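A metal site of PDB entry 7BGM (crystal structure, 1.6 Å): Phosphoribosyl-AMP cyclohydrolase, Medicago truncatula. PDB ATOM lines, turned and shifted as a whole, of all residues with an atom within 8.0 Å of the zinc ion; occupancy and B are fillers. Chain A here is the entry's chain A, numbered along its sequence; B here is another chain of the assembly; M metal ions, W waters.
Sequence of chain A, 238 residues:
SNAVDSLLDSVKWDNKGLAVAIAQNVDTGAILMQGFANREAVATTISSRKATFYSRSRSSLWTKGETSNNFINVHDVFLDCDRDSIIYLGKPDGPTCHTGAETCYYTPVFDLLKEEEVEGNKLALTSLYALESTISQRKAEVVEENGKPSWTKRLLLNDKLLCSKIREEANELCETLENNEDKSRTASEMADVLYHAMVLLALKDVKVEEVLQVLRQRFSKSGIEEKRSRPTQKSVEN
O of Asp 192 sits at hydrogen-bond distance from ND1 of His 196 (2.8 Å). The side-chain carboxylate (OE2) of Glu 189 lies within salt-bridge range of the guanidinium group (NH1) of Arg 185, 2.7 Å away. The side-chain carboxylate of Glu 169 is in salt-bridge range of the side-chain amino group of Lys 165, 3.1 Å away. The side-chain carboxylate (OD1) of Asp 192 lies within salt-bridge range of the guanidinium group (NH1) of Arg 218 of chain B (2.7 Å).
Three residues have an atom within 4 Å of the zinc ion: Glu 169, Glu 189 and Asp 192.
The zinc ion is bound by OE1 of Glu 189, OD2 of Asp 192, OE1 of Glu 169 and water W1.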
ATOM      1  N   LYS A 165      -8.012   0.619  -8.414  1.00  0.00           N
ATOM      2  CA  LYS A 165      -6.789   0.413  -7.646  1.00  0.00           C
ATOM      3  C   LYS A 165      -5.549   0.908  -8.389  1.00  0.00           C
ATOM      4  O   LYS A 165      -4.645   1.475  -7.783  1.00  0.00           O
ATOM      5  CB  LYS A 165      -6.634  -1.066  -7.289  1.00  0.00           C
ATOM      6  CG  LYS A 165      -7.619  -1.572  -6.214  1.00  0.00           C
ATOM      7  CD  LYS A 165      -7.400  -0.897  -4.874  1.00  0.00           C
ATOM      8  CE  LYS A 165      -5.957  -1.018  -4.386  1.00  0.00           C
ATOM      9  NZ  LYS A 165      -5.650  -0.016  -3.308  1.00  0.00           N
ATOM     10  N   GLU A 168      -5.471   4.585  -8.121  1.00  0.00           N
ATOM     11  CA  GLU A 168      -5.182   4.915  -6.719  1.00  0.00           C
ATOM     12  C   GLU A 168      -3.715   4.692  -6.383  1.00  0.00           C
ATOM     13  O   GLU A 168      -3.096   5.531  -5.708  1.00  0.00           O
ATOM     14  CB  GLU A 168      -6.062   4.070  -5.806  1.00  0.00           C
ATOM     15  CG  GLU A 168      -5.521   3.886  -4.387  1.00  0.00           C
ATOM     16  CD  GLU A 168      -6.489   3.154  -3.466  1.00  0.00           C
ATOM     17  OE1 GLU A 168      -7.696   3.499  -3.455  1.00  0.00           O
ATOM     18  OE2 GLU A 168      -6.048   2.233  -2.751  1.00  0.00           O
ATOM     19  N   GLU A 169      -3.153   3.562  -6.828  1.00  0.00           N
ATOM     20  CA  GLU A 169      -1.779   3.224  -6.477  1.00  0.00           C
ATOM     21  C   GLU A 169      -0.778   4.137  -7.181  1.00  0.00           C
ATOM     22  O   GLU A 169       0.275   4.474  -6.617  1.00  0.00           O
ATOM     23  CB  GLU A 169      -1.482   1.763  -6.835  1.00  0.00           C
ATOM     24  CG  GLU A 169      -2.264   0.723  -6.010  1.00  0.00           C
ATOM     25  CD  GLU A 169      -1.925   0.740  -4.534  1.00  0.00           C
ATOM     26  OE1 GLU A 169      -1.007   1.495  -4.139  1.00  0.00           O
ATOM     27  OE2 GLU A 169      -2.582  -0.005  -3.761  1.00  0.00           O
ATOM     28  N   ALA A 170      -1.070   4.495  -8.440  1.00  0.00           N
ATOM     29  CA  ALA A 170      -0.189   5.408  -9.157  1.00  0.00           C
ATOM     30  C   ALA A 170      -0.105   6.744  -8.439  1.00  0.00           C
ATOM     31  O   ALA A 170       0.974   7.353  -8.345  1.00  0.00           O
ATOM     32  CB  ALA A 170      -0.693   5.605 -10.588  1.00  0.00           C
ATOM     33  N   ASN A 171      -1.237   7.217  -7.921  1.00  0.00           N
ATOM     34  CA  ASN A 171      -1.220   8.446  -7.137  1.00  0.00           C
ATOM     35  C   ASN A 171      -0.440   8.283  -5.836  1.00  0.00           C
ATOM     36  O   ASN A 171       0.270   9.214  -5.419  1.00  0.00           O
ATOM     37  CB  ASN A 171      -2.655   8.873  -6.838  1.00  0.00           C
ATOM     38  CG  ASN A 171      -2.717  10.178  -6.084  1.00  0.00           C
ATOM     39  OD1 ASN A 171      -2.324  11.230  -6.605  1.00  0.00           O
ATOM     40  ND2 ASN A 171      -3.205  10.130  -4.848  1.00  0.00           N
ATOM     41  N   GLU A 172      -0.575   7.124  -5.170  1.00  0.00           N
ATOM     42  CA  GLU A 172       0.223   6.848  -3.962  1.00  0.00           C
ATOM     43  C   GLU A 172       1.709   6.918  -4.264  1.00  0.00           C
ATOM     44  O   GLU A 172       2.495   7.459  -3.462  1.00  0.00           O
ATOM     45  CB  GLU A 172      -0.113   5.467  -3.385  1.00  0.00           C
ATOM     46  CG  GLU A 172      -1.476   5.349  -2.738  1.00  0.00           C
ATOM     47  CD  GLU A 172      -1.679   6.341  -1.611  1.00  0.00           C
ATOM     48  OE1 GLU A 172      -0.798   6.454  -0.738  1.00  0.00           O
ATOM     49  OE2 GLU A 172      -2.718   7.016  -1.631  1.00  0.00           O
ATOM     50  N   LEU A 173       2.136   6.332  -5.383  1.00  0.00           N
ATOM     51  CA  LEU A 173       3.549   6.377  -5.748  1.00  0.00           C
ATOM     52  C   LEU A 173       4.004   7.816  -5.956  1.00  0.00           C
ATOM     53  O   LEU A 173       5.082   8.206  -5.477  1.00  0.00           O
ATOM     54  CB  LEU A 173       3.772   5.558  -7.016  1.00  0.00           C
ATOM     55  CG  LEU A 173       5.220   5.505  -7.509  1.00  0.00           C
ATOM     56  CD1 LEU A 173       6.143   4.719  -6.549  1.00  0.00           C
ATOM     57  CD2 LEU A 173       5.223   4.903  -8.913  1.00  0.00           C
ATOM     58  N   THR A 176       4.725   9.717  -2.724  1.00  0.00           N
ATOM     59  CA  THR A 176       5.978   9.457  -2.010  1.00  0.00           C
ATOM     60  C   THR A 176       7.070  10.430  -2.434  1.00  0.00           C
ATOM     61  O   THR A 176       8.001  10.699  -1.650  1.00  0.00           O
ATOM     62  CB  THR A 176       6.467   8.004  -2.200  1.00  0.00           C
ATOM     63  OG1 THR A 176       6.911   7.795  -3.556  1.00  0.00           O
ATOM     64  CG2 THR A 176       5.377   6.991  -1.826  1.00  0.00           C
ATOM     65  N   ARG A 185       8.917   3.692   1.564  1.00  0.00           N
ATOM     66  CA  ARG A 185       7.554   3.914   1.108  1.00  0.00           C
ATOM     67  C   ARG A 185       7.473   3.871  -0.418  1.00  0.00           C
ATOM     68  O   ARG A 185       6.555   3.257  -0.970  1.00  0.00           O
ATOM     69  CB  ARG A 185       7.053   5.260   1.623  1.00  0.00           C
ATOM     70  CG  ARG A 185       6.766   5.252   3.097  1.00  0.00           C
ATOM     71  CD  ARG A 185       5.425   4.589   3.369  1.00  0.00           C
ATOM     72  NE  ARG A 185       4.307   5.370   2.837  1.00  0.00           N
ATOM     73  CZ  ARG A 185       3.501   4.972   1.855  1.00  0.00           C
ATOM     74  NH1 ARG A 185       3.672   3.774   1.292  1.00  0.00           N
ATOM     75  NH2 ARG A 185       2.508   5.765   1.452  1.00  0.00           N
ATOM     76  N   SER A 188       7.615   0.308  -1.581  1.00  0.00           N
ATOM     77  CA  SER A 188       6.383  -0.390  -1.269  1.00  0.00           C
ATOM     78  C   SER A 188       5.256   0.031  -2.205  1.00  0.00           C
ATOM     79  O   SER A 188       4.467  -0.807  -2.656  1.00  0.00           O
ATOM     80  CB  SER A 188       6.004  -0.119   0.188  1.00  0.00           C
ATOM     81  OG  SER A 188       4.828  -0.802   0.502  1.00  0.00           O
ATOM     82  N   GLU A 189       5.174   1.323  -2.527  1.00  0.00           N
ATOM     83  CA  GLU A 189       4.118   1.780  -3.440  1.00  0.00           C
ATOM     84  C   GLU A 189       4.386   1.326  -4.870  1.00  0.00           C
ATOM     85  O   GLU A 189       3.441   0.997  -5.605  1.00  0.00           O
ATOM     86  CB  GLU A 189       3.984   3.299  -3.369  1.00  0.00           C
ATOM     87  CG  GLU A 189       3.402   3.738  -2.024  1.00  0.00           C
ATOM     88  CD  GLU A 189       2.107   2.993  -1.674  1.00  0.00           C
ATOM     89  OE1 GLU A 189       1.307   2.709  -2.582  1.00  0.00           O
ATOM     90  OE2 GLU A 189       1.888   2.678  -0.484  1.00  0.00           O
ATOM     91  N   MET A 190       5.652   1.299  -5.294  1.00  0.00           N
ATOM     92  CA  MET A 190       5.963   0.751  -6.618  1.00  0.00           C
ATOM     93  C   MET A 190       5.569  -0.715  -6.712  1.00  0.00           C
ATOM     94  O   MET A 190       5.100  -1.171  -7.761  1.00  0.00           O
ATOM     95  CB  MET A 190       7.447   0.896  -6.930  1.00  0.00           C
ATOM     96  CG  MET A 190       7.821   0.445  -8.347  1.00  0.00           C
ATOM     97  SD  MET A 190       7.153   1.551  -9.609  1.00  0.00           S
ATOM     98  CE  MET A 190       7.696   0.668 -11.069  1.00  0.00           C
ATOM     99  N   ALA A 191       5.736  -1.469  -5.622  1.00  0.00           N
ATOM    100  CA  ALA A 191       5.311  -2.869  -5.657  1.00  0.00           C
ATOM    101  C   ALA A 191       3.797  -2.969  -5.791  1.00  0.00           C
ATOM    102  O   ALA A 191       3.292  -3.857  -6.497  1.00  0.00           O
ATOM    103  CB  ALA A 191       5.798  -3.612  -4.407  1.00  0.00           C
ATOM    104  N   ASP A 192       3.054  -2.041  -5.170  1.00  0.00           N
ATOM    105  CA  ASP A 192       1.591  -1.994  -5.320  1.00  0.00           C
ATOM    106  C   ASP A 192       1.200  -1.694  -6.759  1.00  0.00           C
ATOM    107  O   ASP A 192       0.288  -2.314  -7.313  1.00  0.00           O
ATOM    108  CB  ASP A 192       0.979  -0.924  -4.412  1.00  0.00           C
ATOM    109  CG  ASP A 192       1.053  -1.255  -2.933  1.00  0.00           C
ATOM    110  OD1 ASP A 192       1.509  -2.343  -2.556  1.00  0.00           O
ATOM    111  OD2 ASP A 192       0.633  -0.366  -2.129  1.00  0.00           O
ATOM    112  N   VAL A 193       1.868  -0.712  -7.369  1.00  0.00           N
ATOM    113  CA  VAL A 193       1.602  -0.370  -8.764  1.00  0.00           C
ATOM    114  C   VAL A 193       1.866  -1.571  -9.649  1.00  0.00           C
ATOM    115  O   VAL A 193       1.034  -1.940 -10.488  1.00  0.00           O
ATOM    116  CB  VAL A 193       2.443   0.848  -9.195  1.00  0.00           C
ATOM    117  CG1 VAL A 193       2.324   1.083 -10.699  1.00  0.00           C
ATOM    118  CG2 VAL A 193       2.008   2.090  -8.432  1.00  0.00           C
ATOM    119  N   HIS A 196      -0.823  -4.544  -9.270  1.00  0.00           N
ATOM    120  CA  HIS A 196      -2.129  -4.288  -9.871  1.00  0.00           C
ATOM    121  C   HIS A 196      -2.024  -4.141 -11.390  1.00  0.00           C
ATOM    122  O   HIS A 196      -2.877  -4.642 -12.127  1.00  0.00           O
ATOM    123  CB  HIS A 196      -2.768  -3.055  -9.223  1.00  0.00           C
ATOM    124  CG  HIS A 196      -3.195  -3.290  -7.811  1.00  0.00           C
ATOM    125  ND1 HIS A 196      -2.377  -3.045  -6.731  1.00  0.00           N
ATOM    126  CD2 HIS A 196      -4.358  -3.789  -7.303  1.00  0.00           C
ATOM    127  CE1 HIS A 196      -3.023  -3.364  -5.612  1.00  0.00           C
ATOM    128  NE2 HIS A 196      -4.224  -3.815  -5.935  1.00  0.00           N
ATOM    129  N   ARG B 218       6.069 -10.415  -0.135  1.00  0.00           N
ATOM    130  CA  ARG B 218       4.627 -10.440   0.081  1.00  0.00           C
ATOM    131  C   ARG B 218       3.996 -11.771  -0.309  1.00  0.00           C
ATOM    132  O   ARG B 218       3.024 -12.205   0.326  1.00  0.00           O
ATOM    133  CB  ARG B 218       3.967  -9.324  -0.702  1.00  0.00           C
ATOM    134  CG  ARG B 218       4.430  -7.994  -0.254  1.00  0.00           C
ATOM    135  CD  ARG B 218       3.606  -6.908  -0.881  1.00  0.00           C
ATOM    136  NE  ARG B 218       4.006  -5.603  -0.374  1.00  0.00           N
ATOM    137  CZ  ARG B 218       3.723  -4.462  -0.995  1.00  0.00           C
ATOM    138  NH1 ARG B 218       3.069  -4.501  -2.141  1.00  0.00           N
ATOM    139  NH2 ARG B 218       4.114  -3.307  -0.467  1.00  0.00           N
HETATM  140 ZN    ZN M   1      -0.192   1.448  -2.287  1.00  0.00          ZN
HETATM  141  O   HOH W   1      -1.452   2.060  -0.730  1.00  0.00           O
